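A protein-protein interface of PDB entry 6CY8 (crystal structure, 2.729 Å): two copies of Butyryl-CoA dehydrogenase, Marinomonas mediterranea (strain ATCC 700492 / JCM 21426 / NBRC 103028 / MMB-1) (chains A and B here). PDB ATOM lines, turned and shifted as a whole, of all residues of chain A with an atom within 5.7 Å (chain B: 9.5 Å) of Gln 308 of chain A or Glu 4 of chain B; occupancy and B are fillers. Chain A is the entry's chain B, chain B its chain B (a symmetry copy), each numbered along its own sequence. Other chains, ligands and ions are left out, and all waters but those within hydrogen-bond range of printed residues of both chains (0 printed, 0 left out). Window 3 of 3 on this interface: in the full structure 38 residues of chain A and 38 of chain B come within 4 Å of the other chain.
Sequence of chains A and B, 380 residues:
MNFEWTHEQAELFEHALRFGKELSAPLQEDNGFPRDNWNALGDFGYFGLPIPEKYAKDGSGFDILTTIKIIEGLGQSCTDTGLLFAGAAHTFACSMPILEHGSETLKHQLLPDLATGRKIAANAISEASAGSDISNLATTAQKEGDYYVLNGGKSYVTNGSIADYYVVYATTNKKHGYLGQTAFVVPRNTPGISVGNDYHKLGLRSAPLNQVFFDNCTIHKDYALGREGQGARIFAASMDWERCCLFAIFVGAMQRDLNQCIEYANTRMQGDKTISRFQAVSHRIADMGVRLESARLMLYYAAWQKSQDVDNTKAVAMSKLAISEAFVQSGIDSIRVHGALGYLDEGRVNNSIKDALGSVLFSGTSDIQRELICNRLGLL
OD1 of Asn 2 of chain B is in hydrogen-bond range of N of Met 1 of chain A (3.2 Å).
The backbone NH (N) of Met 1 of chain A lies within hydrogen-bond range of the backbone carbonyl oxygen (O) of Glu 4 of chain B, 2.5 Å away.
The side-chain amide oxygen (OD1) of Asn 2 of chain A is in hydrogen-bond range of the backbone NH (N) of Met 1 of chain B (3.2 Å).
ND2 of Asn 2 of chain B lies close to ND2 of Asn 2 of chain A (2.7 Å).
N of Phe 3 of chain B sits close to NE1 of Trp 304 of chain A (3.4 Å).
The side-chain amide oxygen (OD1) of Asn 2 of chain B is in hydrogen-bond range of the backbone NH (N) of Glu 4 of chain B (2.9 Å).
The side-chain hydroxyl of Tyr 300 of chain B lies within hydrogen-bond range of the side-chain amino group of Lys 69 of chain B (3.0 Å).
Among the printed residues, pairs that only touch across the chains: Met 1 of chain A with Phe 3 of chain B, Met 1 of chain A with Trp 5 of chain B, Met 1 of chain A with Leu 65 of chain B, Met 1 of chain A with Tyr 300 of chain B, Trp 304 of chain A with Asn 2 of chain B, Trp 304 of chain A with Glu 4 of chain B and Gln 308 of chain A with Glu 4 of chain B.
Of the printed residues of chain B, Trp 304 of chain A touches Asn 2, Phe 3 and Glu 4.
Ser 307 of chain A touches none of the printed residues of chain B.
Of chain B, only Glu 4 comes within 4 Å of Gln 308 of chain A.
No residue of chain B comes within 4 Å of Asp 309 of chain A.
Of the printed residues of chain A, Met 1 of chain B touches Asn 2 (3.2 Å).
Glu 4 of chain B touches just these residues of chain A: Met 1, Trp 304 and Gln 308.
Printed residues of chain A within 4 Å of Trp 5 of chain B: Met 1 (3.5 Å).
The nearest printed residue of chain B that does not touch Asn 2 of chain A is Phe 3 of chain B (5.2 Å).
Hydrophobic or aromatic side chains of chain B within 4 Å of the printed part of chain A: Phe 3, Trp 5, Leu 65 and Tyr 300.
Hydrophobic or aromatic side chains of chain A within 4 Å of the printed part of chain B: Met 1 and Trp 304.
Among the printed residues, 12 pairs touch across the chains.
Among the printed residues, no Asp or Glu carboxylate lies within 4 Å of a Lys or Arg side-chain nitrogen of the other chain.
Met 1 of chain A touches Asn 2 of chain B, and with the chains exchanged Asn 2 of chain A touches Met 1 of chain B.
Asn 2 of chain A touches its own counterpart, Asn 2 of chain B.
2 positions are printed for both chains.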
ATOM      1  N   MET A   1      -4.483   8.792   2.322  1.00  0.00           N
ATOM      2  CA  MET A   1      -4.396   9.680   1.167  1.00  0.00           C
ATOM      3  C   MET A   1      -3.247   9.298   0.226  1.00  0.00           C
ATOM      4  O   MET A   1      -2.106   9.719   0.431  1.00  0.00           O
ATOM      5  CB  MET A   1      -4.227  11.122   1.639  1.00  0.00           C
ATOM      6  CG  MET A   1      -4.066  12.146   0.521  1.00  0.00           C
ATOM      7  SD  MET A   1      -5.578  12.517  -0.381  1.00  0.00           S
ATOM      8  CE  MET A   1      -6.715  12.933   0.950  1.00  0.00           C
ATOM      9  N   ASN A   2      -3.549   8.489  -0.790  1.00  0.00           N
ATOM     10  CA  ASN A   2      -2.591   8.153  -1.838  1.00  0.00           C
ATOM     11  C   ASN A   2      -3.348   7.877  -3.135  1.00  0.00           C
ATOM     12  O   ASN A   2      -4.547   7.598  -3.132  1.00  0.00           O
ATOM     13  CB  ASN A   2      -1.722   6.945  -1.461  1.00  0.00           C
ATOM     14  CG  ASN A   2      -2.438   5.611  -1.682  1.00  0.00           C
ATOM     15  OD1 ASN A   2      -2.319   4.995  -2.738  1.00  0.00           O
ATOM     16  ND2 ASN A   2      -3.193   5.177  -0.695  1.00  0.00           N
ATOM     17  N   TRP A 304     -14.535   6.555  -4.263  1.00  0.00           N
ATOM     18  CA  TRP A 304     -14.019   6.248  -2.934  1.00  0.00           C
ATOM     19  C   TRP A 304     -15.035   6.586  -1.848  1.00  0.00           C
ATOM     20  O   TRP A 304     -15.304   5.761  -0.966  1.00  0.00           O
ATOM     21  CB  TRP A 304     -12.713   7.002  -2.693  1.00  0.00           C
ATOM     22  CG  TRP A 304     -12.196   6.858  -1.293  1.00  0.00           C
ATOM     23  CD1 TRP A 304     -11.400   5.855  -0.815  1.00  0.00           C
ATOM     24  CD2 TRP A 304     -12.420   7.750  -0.201  1.00  0.00           C
ATOM     25  NE1 TRP A 304     -11.120   6.065   0.511  1.00  0.00           N
ATOM     26  CE2 TRP A 304     -11.736   7.219   0.917  1.00  0.00           C
ATOM     27  CE3 TRP A 304     -13.124   8.948  -0.055  1.00  0.00           C
ATOM     28  CZ2 TRP A 304     -11.737   7.845   2.168  1.00  0.00           C
ATOM     29  CZ3 TRP A 304     -13.134   9.568   1.198  1.00  0.00           C
ATOM     30  CH2 TRP A 304     -12.441   9.015   2.289  1.00  0.00           C
ATOM     31  N   GLN A 305     -15.608   7.797  -1.883  1.00  0.00           N
ATOM     32  CA  GLN A 305     -16.591   8.146  -0.861  1.00  0.00           C
ATOM     33  C   GLN A 305     -17.771   7.184  -0.870  1.00  0.00           C
ATOM     34  O   GLN A 305     -18.350   6.906   0.183  1.00  0.00           O
ATOM     35  CB  GLN A 305     -17.091   9.591  -1.025  1.00  0.00           C
ATOM     36  CG  GLN A 305     -16.275  10.633  -0.261  1.00  0.00           C
ATOM     37  CD  GLN A 305     -17.103  11.828   0.220  1.00  0.00           C
ATOM     38  OE1 GLN A 305     -16.716  12.533   1.149  1.00  0.00           O
ATOM     39  NE2 GLN A 305     -18.245  12.046  -0.404  1.00  0.00           N
ATOM     40  N   LYS A 306     -18.141   6.675  -2.044  1.00  0.00           N
ATOM     41  CA  LYS A 306     -19.292   5.787  -2.139  1.00  0.00           C
ATOM     42  C   LYS A 306     -19.057   4.476  -1.391  1.00  0.00           C
ATOM     43  O   LYS A 306     -20.013   3.874  -0.889  1.00  0.00           O
ATOM     44  CB  LYS A 306     -19.627   5.536  -3.609  1.00  0.00           C
ATOM     45  CG  LYS A 306     -21.033   5.026  -3.842  1.00  0.00           C
ATOM     46  CD  LYS A 306     -21.290   4.731  -5.312  1.00  0.00           C
ATOM     47  CE  LYS A 306     -22.499   3.819  -5.478  1.00  0.00           C
ATOM     48  NZ  LYS A 306     -23.701   4.359  -4.771  1.00  0.00           N
ATOM     49  N   SER A 307     -17.804   4.036  -1.292  1.00  0.00           N
ATOM     50  CA  SER A 307     -17.400   2.854  -0.543  1.00  0.00           C
ATOM     51  C   SER A 307     -17.215   3.117   0.949  1.00  0.00           C
ATOM     52  O   SER A 307     -16.707   2.232   1.639  1.00  0.00           O
ATOM     53  CB  SER A 307     -16.074   2.313  -1.086  1.00  0.00           C
ATOM     54  OG  SER A 307     -16.040   2.274  -2.498  1.00  0.00           O
ATOM     55  N   GLN A 308     -17.586   4.297   1.457  1.00  0.00           N
ATOM     56  CA  GLN A 308     -17.124   4.770   2.755  1.00  0.00           C
ATOM     57  C   GLN A 308     -18.216   4.961   3.789  1.00  0.00           C
ATOM     58  O   GLN A 308     -17.891   5.264   4.944  1.00  0.00           O
ATOM     59  CB  GLN A 308     -16.380   6.111   2.620  1.00  0.00           C
ATOM     60  CG  GLN A 308     -14.979   6.006   2.094  1.00  0.00           C
ATOM     61  CD  GLN A 308     -14.195   4.955   2.818  1.00  0.00           C
ATOM     62  OE1 GLN A 308     -14.072   5.004   4.041  1.00  0.00           O
ATOM     63  NE2 GLN A 308     -13.656   3.983   2.071  1.00  0.00           N
ATOM     64  N   ASP A 309     -19.484   4.831   3.417  1.00  0.00           N
ATOM     65  CA  ASP A 309     -20.603   5.059   4.335  1.00  0.00           C
ATOM     66  C   ASP A 309     -20.581   6.480   4.909  1.00  0.00           C
ATOM     67  O   ASP A 309     -20.405   6.713   6.110  1.00  0.00           O
ATOM     68  CB  ASP A 309     -20.635   4.017   5.457  1.00  0.00           C
ATOM     69  CG  ASP A 309     -21.975   3.977   6.158  1.00  0.00           C
ATOM     70  OD1 ASP A 309     -22.944   4.537   5.594  1.00  0.00           O
ATOM     71  OD2 ASP A 309     -22.063   3.401   7.267  1.00  0.00           O
ATOM     72  N   VAL A 310     -20.745   7.432   4.001  1.00  0.00           N
ATOM     73  CA  VAL A 310     -21.152   8.797   4.301  1.00  0.00           C
ATOM     74  C   VAL A 310     -22.105   9.189   3.182  1.00  0.00           C
ATOM     75  O   VAL A 310     -22.292   8.445   2.219  1.00  0.00           O
ATOM     76  CB  VAL A 310     -19.958   9.769   4.372  1.00  0.00           C
ATOM     77  CG1 VAL A 310     -19.138   9.524   5.627  1.00  0.00           C
ATOM     78  CG2 VAL A 310     -19.093   9.622   3.115  1.00  0.00           C
ATOM     79  N   MET B   1      -5.111   3.823  -3.755  1.00  0.00           N
ATOM     80  CA  MET B   1      -6.085   4.859  -4.082  1.00  0.00           C
ATOM     81  C   MET B   1      -7.139   5.034  -2.982  1.00  0.00           C
ATOM     82  O   MET B   1      -8.146   4.322  -2.963  1.00  0.00           O
ATOM     83  CB  MET B   1      -6.764   4.526  -5.409  1.00  0.00           C
ATOM     84  CG  MET B   1      -7.849   5.508  -5.835  1.00  0.00           C
ATOM     85  SD  MET B   1      -7.236   7.089  -6.437  1.00  0.00           S
ATOM     86  CE  MET B   1      -6.055   6.579  -7.694  1.00  0.00           C
ATOM     87  N   ASN B   2      -6.894   5.969  -2.063  1.00  0.00           N
ATOM     88  CA  ASN B   2      -7.868   6.338  -1.040  1.00  0.00           C
ATOM     89  C   ASN B   2      -7.658   7.801  -0.658  1.00  0.00           C
ATOM     90  O   ASN B   2      -6.596   8.380  -0.891  1.00  0.00           O
ATOM     91  CB  ASN B   2      -7.768   5.442   0.203  1.00  0.00           C
ATOM     92  CG  ASN B   2      -6.627   5.853   1.135  1.00  0.00           C
ATOM     93  OD1 ASN B   2      -6.818   6.626   2.070  1.00  0.00           O
ATOM     94  ND2 ASN B   2      -5.439   5.349   0.870  1.00  0.00           N
ATOM     95  N   PHE B   3      -8.681   8.385  -0.046  1.00  0.00           N
ATOM     96  CA  PHE B   3      -8.683   9.796   0.316  1.00  0.00           C
ATOM     97  C   PHE B   3      -8.803   9.986   1.827  1.00  0.00           C
ATOM     98  O   PHE B   3      -9.329  10.994   2.304  1.00  0.00           O
ATOM     99  CB  PHE B   3      -9.797  10.521  -0.445  1.00  0.00           C
ATOM    100  CG  PHE B   3      -9.576  10.535  -1.944  1.00  0.00           C
ATOM    101  CD1 PHE B   3      -9.996   9.475  -2.732  1.00  0.00           C
ATOM    102  CD2 PHE B   3      -8.898  11.582  -2.549  1.00  0.00           C
ATOM    103  CE1 PHE B   3      -9.767   9.477  -4.096  1.00  0.00           C
ATOM    104  CE2 PHE B   3      -8.667  11.589  -3.914  1.00  0.00           C
ATOM    105  CZ  PHE B   3      -9.101  10.534  -4.687  1.00  0.00           C
ATOM    106  N   GLU B   4      -8.288   9.023   2.586  1.00  0.00           N
ATOM    107  CA  GLU B   4      -8.372   9.009   4.041  1.00  0.00           C
ATOM    108  C   GLU B   4      -7.103   9.618   4.625  1.00  0.00           C
ATOM    109  O   GLU B   4      -5.992   9.239   4.234  1.00  0.00           O
ATOM    110  CB  GLU B   4      -8.557   7.570   4.550  1.00  0.00           C
ATOM    111  CG  GLU B   4      -9.200   7.403   5.944  1.00  0.00           C
ATOM    112  CD  GLU B   4     -10.567   8.079   6.059  1.00  0.00           C
ATOM    113  OE1 GLU B   4     -10.628   9.316   6.278  1.00  0.00           O
ATOM    114  OE2 GLU B   4     -11.588   7.360   5.929  1.00  0.00           O
ATOM    115  N   TRP B   5      -7.268  10.574   5.537  1.00  0.00           N
ATOM    116  CA  TRP B   5      -6.155  11.091   6.325  1.00  0.00           C
ATOM    117  C   TRP B   5      -6.019  10.270   7.602  1.00  0.00           C
ATOM    118  O   TRP B   5      -7.021   9.864   8.194  1.00  0.00           O
ATOM    119  CB  TRP B   5      -6.356  12.572   6.688  1.00  0.00           C
ATOM    120  CG  TRP B   5      -6.464  13.509   5.522  1.00  0.00           C
ATOM    121  CD1 TRP B   5      -7.604  13.947   4.902  1.00  0.00           C
ATOM    122  CD2 TRP B   5      -5.371  14.082   4.796  1.00  0.00           C
ATOM    123  NE1 TRP B   5      -7.281  14.783   3.853  1.00  0.00           N
ATOM    124  CE2 TRP B   5      -5.916  14.873   3.761  1.00  0.00           C
ATOM    125  CE3 TRP B   5      -3.984  14.007   4.930  1.00  0.00           C
ATOM    126  CZ2 TRP B   5      -5.118  15.584   2.868  1.00  0.00           C
ATOM    127  CZ3 TRP B   5      -3.197  14.708   4.054  1.00  0.00           C
ATOM    128  CH2 TRP B   5      -3.760  15.498   3.034  1.00  0.00           C
ATOM    129  N   THR B   6      -4.777  10.041   8.024  1.00  0.00           N
ATOM    130  CA  THR B   6      -4.525   9.360   9.288  1.00  0.00           C
ATOM    131  C   THR B   6      -5.077  10.172  10.452  1.00  0.00           C
ATOM    132  O   THR B   6      -5.313  11.379  10.348  1.00  0.00           O
ATOM    133  CB  THR B   6      -3.024   9.130   9.530  1.00  0.00           C
ATOM    134  OG1 THR B   6      -2.399  10.367   9.911  1.00  0.00           O
ATOM    135  CG2 THR B   6      -2.319   8.539   8.293  1.00  0.00           C
ATOM    136  N   HIS B   7      -5.293   9.480  11.577  1.00  0.00           N
ATOM    137  CA  HIS B   7      -5.731  10.141  12.806  1.00  0.00           C
ATOM    138  C   HIS B   7      -4.831  11.327  13.132  1.00  0.00           C
ATOM    139  O   HIS B   7      -5.309  12.419  13.467  1.00  0.00           O
ATOM    140  CB  HIS B   7      -5.734   9.121  13.955  1.00  0.00           C
ATOM    141  CG  HIS B   7      -6.588   9.509  15.124  1.00  0.00           C
ATOM    142  ND1 HIS B   7      -7.832   8.957  15.354  1.00  0.00           N
ATOM    143  CD2 HIS B   7      -6.360  10.367  16.150  1.00  0.00           C
ATOM    144  CE1 HIS B   7      -8.343   9.472  16.459  1.00  0.00           C
ATOM    145  NE2 HIS B   7      -7.471  10.331  16.961  1.00  0.00           N
ATOM    146  N   GLU B   8      -3.518  11.133  13.005  1.00  0.00           N
ATOM    147  CA  GLU B   8      -2.549  12.180  13.311  1.00  0.00           C
ATOM    148  C   GLU B   8      -2.673  13.363  12.347  1.00  0.00           C
ATOM    149  O   GLU B   8      -2.524  14.526  12.747  1.00  0.00           O
ATOM    150  CB  GLU B   8      -1.147  11.561  13.275  1.00  0.00           C
ATOM    151  CG  GLU B   8       0.004  12.507  13.024  1.00  0.00           C
ATOM    152  CD  GLU B   8       0.737  12.882  14.298  1.00  0.00           C
ATOM    153  OE1 GLU B   8       0.252  12.509  15.393  1.00  0.00           O
ATOM    154  OE2 GLU B   8       1.804  13.537  14.199  1.00  0.00           O
ATOM    155  N   GLN B   9      -2.958  13.090  11.074  1.00  0.00           N
ATOM    156  CA  GLN B   9      -3.104  14.171  10.107  1.00  0.00           C
ATOM    157  C   GLN B   9      -4.366  14.977  10.369  1.00  0.00           C
ATOM    158  O   GLN B   9      -4.329  16.214  10.357  1.00  0.00           O
ATOM    159  CB  GLN B   9      -3.107  13.606   8.697  1.00  0.00           C
ATOM    160  CG  GLN B   9      -1.723  13.414   8.130  1.00  0.00           C
ATOM    161  CD  GLN B   9      -1.726  12.440   6.997  1.00  0.00           C
ATOM    162  OE1 GLN B   9      -2.607  11.570   6.914  1.00  0.00           O
ATOM    163  NE2 GLN B   9      -0.753  12.571   6.102  1.00  0.00           N
ATOM    164  N   ALA B  10      -5.500  14.298  10.593  1.00  0.00           N
ATOM    165  CA  ALA B  10      -6.720  15.010  10.964  1.00  0.00           C
ATOM    166  C   ALA B  10      -6.493  15.894  12.180  1.00  0.00           C
ATOM    167  O   ALA B  10      -7.020  17.012  12.251  1.00  0.00           O
ATOM    168  CB  ALA B  10      -7.857  14.030  11.244  1.00  0.00           C
ATOM    169  N   LEU B  65       2.304  15.841   1.933  1.00  0.00           N
ATOM    170  CA  LEU B  65       0.862  15.862   2.148  1.00  0.00           C
ATOM    171  C   LEU B  65       0.504  16.436   3.513  1.00  0.00           C
ATOM    172  O   LEU B  65      -0.386  17.296   3.616  1.00  0.00           O
ATOM    173  CB  LEU B  65       0.283  14.461   1.982  1.00  0.00           C
ATOM    174  CG  LEU B  65      -0.075  14.102   0.542  1.00  0.00           C
ATOM    175  CD1 LEU B  65      -0.511  12.650   0.468  1.00  0.00           C
ATOM    176  CD2 LEU B  65      -1.154  15.040   0.019  1.00  0.00           C
ATOM    177  N   THR B  66       1.168  15.963   4.578  1.00  0.00           N
ATOM    178  CA  THR B  66       0.918  16.525   5.906  1.00  0.00           C
ATOM    179  C   THR B  66       1.248  18.014   5.934  1.00  0.00           C
ATOM    180  O   THR B  66       0.534  18.814   6.555  1.00  0.00           O
ATOM    181  CB  THR B  66       1.728  15.772   6.972  1.00  0.00           C
ATOM    182  OG1 THR B  66       1.336  14.399   6.991  1.00  0.00           O
ATOM    183  CG2 THR B  66       1.476  16.339   8.356  1.00  0.00           C
ATOM    184  N   LYS B  69      -1.508  19.956   3.941  1.00  0.00           N
ATOM    185  CA  LYS B  69      -2.791  19.872   4.627  1.00  0.00           C
ATOM    186  C   LYS B  69      -2.834  20.828   5.809  1.00  0.00           C
ATOM    187  O   LYS B  69      -3.857  21.479   6.053  1.00  0.00           O
ATOM    188  CB  LYS B  69      -3.051  18.425   5.057  1.00  0.00           C
ATOM    189  CG  LYS B  69      -4.383  18.176   5.756  1.00  0.00           C
ATOM    190  CD  LYS B  69      -5.568  18.441   4.836  1.00  0.00           C
ATOM    191  CE  LYS B  69      -6.851  17.851   5.399  1.00  0.00           C
ATOM    192  NZ  LYS B  69      -8.054  18.306   4.641  1.00  0.00           N
ATOM    193  N   LEU B 297      -8.467  18.641  -4.912  1.00  0.00           N
ATOM    194  CA  LEU B 297      -8.044  17.310  -5.346  1.00  0.00           C
ATOM    195  C   LEU B 297      -6.765  17.374  -6.178  1.00  0.00           C
ATOM    196  O   LEU B 297      -5.868  16.545  -6.006  1.00  0.00           O
ATOM    197  CB  LEU B 297      -9.170  16.626  -6.121  1.00  0.00           C
ATOM    198  CG  LEU B 297     -10.369  16.177  -5.273  1.00  0.00           C
ATOM    199  CD1 LEU B 297     -11.590  15.810  -6.141  1.00  0.00           C
ATOM    200  CD2 LEU B 297      -9.977  15.027  -4.342  1.00  0.00           C
ATOM    201  N   TYR B 300      -3.864  17.930  -3.696  1.00  0.00           N
ATOM    202  CA  TYR B 300      -3.474  16.677  -3.062  1.00  0.00           C
ATOM    203  C   TYR B 300      -2.733  15.780  -4.041  1.00  0.00           C
ATOM    204  O   TYR B 300      -1.664  15.243  -3.721  1.00  0.00           O
ATOM    205  CB  TYR B 300      -4.713  15.962  -2.521  1.00  0.00           C
ATOM    206  CG  TYR B 300      -5.381  16.675  -1.384  1.00  0.00           C
ATOM    207  CD1 TYR B 300      -4.748  17.732  -0.734  1.00  0.00           C
ATOM    208  CD2 TYR B 300      -6.639  16.285  -0.941  1.00  0.00           C
ATOM    209  CE1 TYR B 300      -5.358  18.387   0.334  1.00  0.00           C
ATOM    210  CE2 TYR B 300      -7.258  16.935   0.127  1.00  0.00           C
ATOM    211  CZ  TYR B 300      -6.615  17.984   0.758  1.00  0.00           C
ATOM    212  OH  TYR B 300      -7.243  18.621   1.808  1.00  0.00           O
